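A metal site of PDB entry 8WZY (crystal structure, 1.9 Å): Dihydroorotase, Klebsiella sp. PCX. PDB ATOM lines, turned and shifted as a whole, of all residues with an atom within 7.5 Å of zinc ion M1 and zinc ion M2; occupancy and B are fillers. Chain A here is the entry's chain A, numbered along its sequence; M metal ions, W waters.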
ATOM      1  N   HIS A  56      28.490  19.719  21.636  1.00  0.00           N
ATOM      2  CA  HIS A  56      28.425  20.429  22.905  1.00  0.00           C
ATOM      3  C   HIS A  56      27.618  19.579  23.889  1.00  0.00           C
ATOM      4  O   HIS A  56      26.401  19.744  23.989  1.00  0.00           O
ATOM      5  CB  HIS A  56      27.820  21.810  22.747  1.00  0.00           C
ATOM      6  CG  HIS A  56      27.891  22.653  23.973  1.00  0.00           C
ATOM      7  ND1 HIS A  56      27.904  24.026  23.938  1.00  0.00           N
ATOM      8  CD2 HIS A  56      27.959  22.309  25.288  1.00  0.00           C
ATOM      9  CE1 HIS A  56      27.988  24.497  25.170  1.00  0.00           C
ATOM     10  NE2 HIS A  56      28.015  23.476  26.008  1.00  0.00           N
ATOM     11  N   VAL A  57      28.293  18.678  24.586  1.00  0.00           N
ATOM     12  CA  VAL A  57      27.667  17.863  25.620  1.00  0.00           C
ATOM     13  C   VAL A  57      28.501  17.974  26.891  1.00  0.00           C
ATOM     14  O   VAL A  57      29.609  18.498  26.888  1.00  0.00           O
ATOM     15  CB  VAL A  57      27.528  16.385  25.222  1.00  0.00           C
ATOM     16  CG1 VAL A  57      26.785  16.232  23.896  1.00  0.00           C
ATOM     17  CG2 VAL A  57      28.901  15.690  25.203  1.00  0.00           C
ATOM     18  N   HIS A  58      27.947  17.441  27.977  1.00  0.00           N
ATOM     19  CA  HIS A  58      28.697  17.215  29.216  1.00  0.00           C
ATOM     20  C   HIS A  58      28.513  15.768  29.630  1.00  0.00           C
ATOM     21  O   HIS A  58      27.489  15.409  30.221  1.00  0.00           O
ATOM     22  CB  HIS A  58      28.259  18.171  30.310  1.00  0.00           C
ATOM     23  CG  HIS A  58      28.545  19.585  29.979  1.00  0.00           C
ATOM     24  ND1 HIS A  58      29.824  20.087  29.951  1.00  0.00           N
ATOM     25  CD2 HIS A  58      27.732  20.586  29.572  1.00  0.00           C
ATOM     26  CE1 HIS A  58      29.787  21.357  29.578  1.00  0.00           C
ATOM     27  NE2 HIS A  58      28.529  21.678  29.350  1.00  0.00           N
ATOM     28  N   TYR A  66      27.315  19.043  36.098  1.00  0.00           N
ATOM     29  CA  TYR A  66      26.960  18.746  34.714  1.00  0.00           C
ATOM     30  C   TYR A  66      27.655  17.446  34.323  1.00  0.00           C
ATOM     31  O   TYR A  66      28.730  17.443  33.724  1.00  0.00           O
ATOM     32  CB  TYR A  66      27.306  19.911  33.804  1.00  0.00           C
ATOM     33  CG  TYR A  66      26.853  21.226  34.383  1.00  0.00           C
ATOM     34  CD1 TYR A  66      25.523  21.603  34.311  1.00  0.00           C
ATOM     35  CD2 TYR A  66      27.757  22.096  34.998  1.00  0.00           C
ATOM     36  CE1 TYR A  66      25.092  22.802  34.862  1.00  0.00           C
ATOM     37  CE2 TYR A  66      27.332  23.291  35.533  1.00  0.00           C
ATOM     38  CZ  TYR A  66      26.000  23.645  35.465  1.00  0.00           C
ATOM     39  OH  TYR A  66      25.554  24.830  35.994  1.00  0.00           O
ATOM     40  N   ASP A  84      32.610  16.698  24.450  1.00  0.00           N
ATOM     41  CA  ASP A  84      32.432  17.275  25.764  1.00  0.00           C
ATOM     42  C   ASP A  84      32.986  18.692  25.790  1.00  0.00           C
ATOM     43  O   ASP A  84      34.148  18.919  25.446  1.00  0.00           O
ATOM     44  CB  ASP A  84      33.112  16.405  26.828  1.00  0.00           C
ATOM     45  CG  ASP A  84      32.977  16.980  28.238  1.00  0.00           C
ATOM     46  OD1 ASP A  84      31.941  16.745  28.893  1.00  0.00           O
ATOM     47  OD2 ASP A  84      33.915  17.675  28.681  1.00  0.00           O
ATOM     48  N   ALA A  85      32.151  19.628  26.220  1.00  0.00           N
ATOM     49  CA  ALA A  85      32.442  21.060  26.054  1.00  0.00           C
ATOM     50  C   ALA A  85      33.113  21.604  27.314  1.00  0.00           C
ATOM     51  O   ALA A  85      32.593  22.455  28.037  1.00  0.00           O
ATOM     52  CB  ALA A  85      31.164  21.818  25.721  1.00  0.00           C
ATOM     53  N   GLY A  86      34.319  21.092  27.561  1.00  0.00           N
ATOM     54  CA  GLY A  86      35.108  21.601  28.654  1.00  0.00           C
ATOM     55  C   GLY A  86      34.624  21.264  30.047  1.00  0.00           C
ATOM     56  O   GLY A  86      34.766  22.091  30.949  1.00  0.00           O
ATOM     57  N   SER A  87      34.055  20.058  30.244  1.00  0.00           N
ATOM     58  CA  SER A  87      33.743  19.605  31.600  1.00  0.00           C
ATOM     59  C   SER A  87      35.010  19.404  32.420  1.00  0.00           C
ATOM     60  O   SER A  87      35.007  19.617  33.639  1.00  0.00           O
ATOM     61  CB  SER A  87      32.944  18.300  31.549  1.00  0.00           C
ATOM     62  OG  SER A  87      31.765  18.435  30.781  1.00  0.00           O
ATOM     63  N   LEU A 118      34.822  22.017  35.117  1.00  0.00           N
ATOM     64  CA  LEU A 118      33.542  22.344  35.718  1.00  0.00           C
ATOM     65  C   LEU A 118      33.401  21.759  37.124  1.00  0.00           C
ATOM     66  O   LEU A 118      32.262  21.558  37.594  1.00  0.00           O
ATOM     67  CB  LEU A 118      32.391  21.891  34.823  1.00  0.00           C
ATOM     68  CG  LEU A 118      32.362  22.591  33.453  1.00  0.00           C
ATOM     69  CD1 LEU A 118      31.156  22.172  32.617  1.00  0.00           C
ATOM     70  CD2 LEU A 118      32.426  24.104  33.620  1.00  0.00           C
ATOM     71  N   KCX A 150      37.838  25.161  25.476  1.00  0.00           N
ATOM     72  CA  KCX A 150      36.551  25.714  25.876  1.00  0.00           C
ATOM     73  CB  KCX A 150      35.682  24.654  26.567  1.00  0.00           C
ATOM     74  CG  KCX A 150      34.163  24.728  26.302  1.00  0.00           C
ATOM     75  CD  KCX A 150      33.547  26.053  26.657  1.00  0.00           C
ATOM     76  CE  KCX A 150      32.049  26.063  26.370  1.00  0.00           C
ATOM     77  NZ  KCX A 150      31.377  25.105  27.314  1.00  0.00           N
ATOM     78  C   KCX A 150      36.771  26.898  26.809  1.00  0.00           C
ATOM     79  O   KCX A 150      37.531  26.790  27.777  1.00  0.00           O
ATOM     80  CX  KCX A 150      30.171  25.301  27.834  1.00  0.00           C
ATOM     81  OQ1 KCX A 150      29.723  24.441  28.614  1.00  0.00           O
ATOM     82  OQ2 KCX A 150      29.484  26.306  27.582  1.00  0.00           O
ATOM     83  N   ALA A 151      36.123  28.016  26.537  1.00  0.00           N
ATOM     84  CA  ALA A 151      36.168  29.141  27.454  1.00  0.00           C
ATOM     85  C   ALA A 151      34.754  29.657  27.699  1.00  0.00           C
ATOM     86  O   ALA A 151      34.078  30.051  26.756  1.00  0.00           O
ATOM     87  CB  ALA A 151      37.064  30.258  26.922  1.00  0.00           C
ATOM     88  N   ARG A 152      34.296  29.623  28.952  1.00  0.00           N
ATOM     89  CA  ARG A 152      32.955  30.098  29.289  1.00  0.00           C
ATOM     90  C   ARG A 152      33.047  31.555  29.724  1.00  0.00           C
ATOM     91  O   ARG A 152      33.337  31.862  30.886  1.00  0.00           O
ATOM     92  CB  ARG A 152      32.321  29.232  30.389  1.00  0.00           C
ATOM     93  CG  ARG A 152      32.283  27.739  30.056  1.00  0.00           C
ATOM     94  CD  ARG A 152      31.247  27.015  30.908  1.00  0.00           C
ATOM     95  NE  ARG A 152      31.551  27.146  32.333  1.00  0.00           N
ATOM     96  CZ  ARG A 152      30.644  27.318  33.280  1.00  0.00           C
ATOM     97  NH1 ARG A 152      29.357  27.396  32.998  1.00  0.00           N
ATOM     98  NH2 ARG A 152      31.050  27.407  34.553  1.00  0.00           N
ATOM     99  N   MET A 153      32.791  32.467  28.793  1.00  0.00           N
ATOM    100  CA  MET A 153      33.054  33.880  29.022  1.00  0.00           C
ATOM    101  C   MET A 153      31.746  34.553  29.419  1.00  0.00           C
ATOM    102  O   MET A 153      31.032  35.103  28.584  1.00  0.00           O
ATOM    103  CB  MET A 153      33.686  34.516  27.793  1.00  0.00           C
ATOM    104  CG  MET A 153      34.956  33.792  27.404  1.00  0.00           C
ATOM    105  SD  MET A 153      36.303  34.233  28.487  1.00  0.00           S
ATOM    106  CE  MET A 153      36.028  35.984  28.739  1.00  0.00           C
ATOM    107  N   SER A 154      31.434  34.501  30.706  1.00  0.00           N
ATOM    108  CA  SER A 154      30.235  35.131  31.235  1.00  0.00           C
ATOM    109  C   SER A 154      30.509  35.584  32.666  1.00  0.00           C
ATOM    110  O   SER A 154      31.553  35.264  33.238  1.00  0.00           O
ATOM    111  CB  SER A 154      29.012  34.209  31.162  1.00  0.00           C
ATOM    112  OG  SER A 154      29.277  32.961  31.780  1.00  0.00           O
ATOM    113  N   VAL A 157      31.463  33.279  35.711  1.00  0.00           N
ATOM    114  CA  VAL A 157      32.593  32.400  35.464  1.00  0.00           C
ATOM    115  C   VAL A 157      33.919  33.144  35.575  1.00  0.00           C
ATOM    116  O   VAL A 157      34.876  32.642  36.163  1.00  0.00           O
ATOM    117  CB  VAL A 157      32.465  31.712  34.089  1.00  0.00           C
ATOM    118  CG1 VAL A 157      33.558  30.663  33.921  1.00  0.00           C
ATOM    119  CG2 VAL A 157      31.088  31.083  33.950  1.00  0.00           C
ATOM    120  N   MET A 182      36.024  27.003  21.489  1.00  0.00           N
ATOM    121  CA  MET A 182      34.605  27.239  21.724  1.00  0.00           C
ATOM    122  C   MET A 182      34.422  28.212  22.878  1.00  0.00           C
ATOM    123  O   MET A 182      34.971  28.017  23.961  1.00  0.00           O
ATOM    124  CB  MET A 182      33.870  25.925  22.021  1.00  0.00           C
ATOM    125  CG  MET A 182      32.404  26.129  22.288  1.00  0.00           C
ATOM    126  SD  MET A 182      31.493  24.594  22.567  1.00  0.00           S
ATOM    127  CE  MET A 182      31.165  24.137  20.870  1.00  0.00           C
ATOM    128  N   VAL A 183      33.654  29.274  22.624  1.00  0.00           N
ATOM    129  CA  VAL A 183      33.446  30.357  23.565  1.00  0.00           C
ATOM    130  C   VAL A 183      31.972  30.372  23.914  1.00  0.00           C
ATOM    131  O   VAL A 183      31.115  30.499  23.029  1.00  0.00           O
ATOM    132  CB  VAL A 183      33.877  31.707  22.963  1.00  0.00           C
ATOM    133  CG1 VAL A 183      33.702  32.822  23.993  1.00  0.00           C
ATOM    134  CG2 VAL A 183      35.323  31.627  22.475  1.00  0.00           C
ATOM    135  N   HIS A 184      31.669  30.202  25.199  1.00  0.00           N
ATOM    136  CA  HIS A 184      30.313  30.322  25.698  1.00  0.00           C
ATOM    137  C   HIS A 184      30.007  31.782  25.982  1.00  0.00           C
ATOM    138  O   HIS A 184      30.870  32.536  26.445  1.00  0.00           O
ATOM    139  CB  HIS A 184      30.146  29.406  26.924  1.00  0.00           C
ATOM    140  CG  HIS A 184      29.471  30.020  28.108  1.00  0.00           C
ATOM    141  ND1 HIS A 184      28.514  29.336  28.838  1.00  0.00           N
ATOM    142  CD2 HIS A 184      29.661  31.184  28.770  1.00  0.00           C
ATOM    143  CE1 HIS A 184      28.116  30.081  29.849  1.00  0.00           C
ATOM    144  NE2 HIS A 184      28.787  31.212  29.833  1.00  0.00           N
ATOM    145  N   ILE A 185      28.775  32.195  25.674  1.00  0.00           N
ATOM    146  CA  ILE A 185      28.302  33.556  25.935  1.00  0.00           C
ATOM    147  C   ILE A 185      26.973  33.476  26.681  1.00  0.00           C
ATOM    148  O   ILE A 185      26.256  32.468  26.624  1.00  0.00           O
ATOM    149  CB  ILE A 185      28.155  34.385  24.639  1.00  0.00           C
ATOM    150  CG1 ILE A 185      27.164  33.705  23.684  1.00  0.00           C
ATOM    151  CG2 ILE A 185      29.508  34.607  23.981  1.00  0.00           C
ATOM    152  CD1 ILE A 185      26.605  34.622  22.597  1.00  0.00           C
ATOM    153  N   THR A 206      29.240  29.409  21.104  1.00  0.00           N
ATOM    154  CA  THR A 206      28.106  28.557  21.456  1.00  0.00           C
ATOM    155  C   THR A 206      27.102  29.339  22.304  1.00  0.00           C
ATOM    156  O   THR A 206      27.350  30.472  22.723  1.00  0.00           O
ATOM    157  CB  THR A 206      28.598  27.283  22.151  1.00  0.00           C
ATOM    158  OG1 THR A 206      27.532  26.328  22.229  1.00  0.00           O
ATOM    159  CG2 THR A 206      29.135  27.582  23.562  1.00  0.00           C
ATOM    160  N   HIS A 207      25.933  28.719  22.539  1.00  0.00           N
ATOM    161  CA  HIS A 207      24.739  29.406  23.065  1.00  0.00           C
ATOM    162  C   HIS A 207      24.333  30.565  22.175  1.00  0.00           C
ATOM    163  O   HIS A 207      23.925  31.624  22.652  1.00  0.00           O
ATOM    164  CB  HIS A 207      24.929  29.873  24.514  1.00  0.00           C
ATOM    165  CG  HIS A 207      25.479  28.829  25.407  1.00  0.00           C
ATOM    166  ND1 HIS A 207      25.071  27.512  25.345  1.00  0.00           N
ATOM    167  CD2 HIS A 207      26.416  28.881  26.383  1.00  0.00           C
ATOM    168  CE1 HIS A 207      25.730  26.806  26.248  1.00  0.00           C
ATOM    169  NE2 HIS A 207      26.540  27.618  26.894  1.00  0.00           N
ATOM    170  N   GLY A 240      24.162  25.055  21.187  1.00  0.00           N
ATOM    171  CA  GLY A 240      24.342  24.738  22.601  1.00  0.00           C
ATOM    172  C   GLY A 240      23.130  25.043  23.452  1.00  0.00           C
ATOM    173  O   GLY A 240      23.231  25.796  24.436  1.00  0.00           O
ATOM    174  N   GLY A 242      21.047  23.847  25.923  1.00  0.00           N
ATOM    175  CA  GLY A 242      21.204  23.924  27.355  1.00  0.00           C
ATOM    176  C   GLY A 242      19.931  24.218  28.113  1.00  0.00           C
ATOM    177  O   GLY A 242      18.820  24.227  27.581  1.00  0.00           O
ATOM    178  N   SER A 245      20.108  28.604  27.681  1.00  0.00           N
ATOM    179  CA  SER A 245      20.869  29.218  26.595  1.00  0.00           C
ATOM    180  C   SER A 245      20.162  29.223  25.244  1.00  0.00           C
ATOM    181  O   SER A 245      20.800  29.536  24.236  1.00  0.00           O
ATOM    182  CB  SER A 245      22.227  28.528  26.435  1.00  0.00           C
ATOM    183  OG  SER A 245      23.041  28.748  27.571  1.00  0.00           O
ATOM    184  N   SER A 266      23.349  20.478  21.775  1.00  0.00           N
ATOM    185  CA  SER A 266      22.316  20.352  22.791  1.00  0.00           C
ATOM    186  C   SER A 266      22.691  20.993  24.121  1.00  0.00           C
ATOM    187  O   SER A 266      21.781  21.433  24.847  1.00  0.00           O
ATOM    188  CB  SER A 266      22.009  18.873  23.038  1.00  0.00           C
ATOM    189  OG  SER A 266      23.177  18.210  23.476  1.00  0.00           O
ATOM    190  N   ASP A 267      23.979  21.056  24.456  1.00  0.00           N
ATOM    191  CA  ASP A 267      24.437  21.414  25.807  1.00  0.00           C
ATOM    192  C   ASP A 267      23.744  20.524  26.842  1.00  0.00           C
ATOM    193  O   ASP A 267      23.244  20.976  27.868  1.00  0.00           O
ATOM    194  CB  ASP A 267      24.218  22.889  26.105  1.00  0.00           C
ATOM    195  CG  ASP A 267      24.879  23.325  27.410  1.00  0.00           C
ATOM    196  OD1 ASP A 267      25.774  22.606  27.898  1.00  0.00           O
ATOM    197  OD2 ASP A 267      24.459  24.360  27.964  1.00  0.00           O
ATOM    198  N   ILE A 268      23.768  19.226  26.556  1.00  0.00           N
ATOM    199  CA  ILE A 268      22.993  18.251  27.306  1.00  0.00           C
ATOM    200  C   ILE A 268      23.824  17.715  28.475  1.00  0.00           C
ATOM    201  O   ILE A 268      25.034  17.529  28.371  1.00  0.00           O
ATOM    202  CB  ILE A 268      22.530  17.124  26.372  1.00  0.00           C
ATOM    203  CG1 ILE A 268      21.476  16.228  27.031  1.00  0.00           C
ATOM    204  CG2 ILE A 268      23.718  16.292  25.876  1.00  0.00           C
ATOM    205  CD1 ILE A 268      20.775  15.297  26.030  1.00  0.00           C
ATOM    206  N   TYR A 269      23.155  17.501  29.602  1.00  0.00           N
ATOM    207  CA  TYR A 269      23.692  16.702  30.685  1.00  0.00           C
ATOM    208  C   TYR A 269      22.517  15.971  31.307  1.00  0.00           C
ATOM    209  O   TYR A 269      21.383  16.103  30.841  1.00  0.00           O
ATOM    210  CB  TYR A 269      24.505  17.548  31.663  1.00  0.00           C
ATOM    211  CG  TYR A 269      23.685  18.393  32.593  1.00  0.00           C
ATOM    212  CD1 TYR A 269      23.055  19.546  32.142  1.00  0.00           C
ATOM    213  CD2 TYR A 269      23.592  18.090  33.946  1.00  0.00           C
ATOM    214  CE1 TYR A 269      22.318  20.332  32.980  1.00  0.00           C
ATOM    215  CE2 TYR A 269      22.861  18.879  34.805  1.00  0.00           C
ATOM    216  CZ  TYR A 269      22.219  19.999  34.324  1.00  0.00           C
ATOM    217  OH  TYR A 269      21.485  20.791  35.175  1.00  0.00           O
HETATM  218 ZN    ZN M   1      27.884  23.520  28.254  1.00  0.00          ZN
HETATM  219 ZN    ZN M   2      27.963  27.143  28.557  1.00  0.00          ZN
HETATM  220  O   HOH W   1      27.469  25.947  31.037  1.00  0.00           O
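O of Ile 268 sits at hydrogen-bond distance from N of His 58.
OG of Ser 87 lies within hydrogen-bond range of ND1 of His 58, 2.7 Å away.
A ring nitrogen (ND1) of His 207 sits close to the side-chain hydroxyl (OG) of Ser 245 (3.3 Å).
A ring nitrogen (ND1) of His 207 sits at hydrogen-bond distance from the backbone carbonyl oxygen of Gly 240, 2.7 Å away.
ND1 of His 56 sits at hydrogen-bond distance from OG1 of Thr 206 (2.9 Å).
NE2 of His 184 lies within hydrogen-bond range of OG of Ser 154, at 2.7 Å.
N of His 184 sits at hydrogen-bond distance from O of Ala 151 (2.9 Å).
O of His 184 sits at hydrogen-bond distance from N of Met 153 (3.0 Å).
Within 4 Å of zinc ion M1: His 56, His 58, KCX 150 and Asp 267.
Three residues have an atom within 4 Å of zinc ion M2: KCX 150, His 184 and His 207.
Zinc ion M1 is bound by OQ1 of KCX 150 (2.1 Å), NE2 of His 58 (2.2 Å), NE2 of His 56 (2.3 Å) and OD1 of Asp 267 (2.3 Å).
Zinc ion M1 has four donor atoms within binding distance.
Zinc ion M2 is bound by OQ2 of KCX 150.
NE2 of His 207 binds zinc ion M2, 2.2 Å away.
ND1 of His 184 binds zinc ion M2, 2.3 Å away.
Zinc ion M2 has three donor atoms within binding distance.
Slightly farther from zinc ion M2 lies water W1 (2.8 Å).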
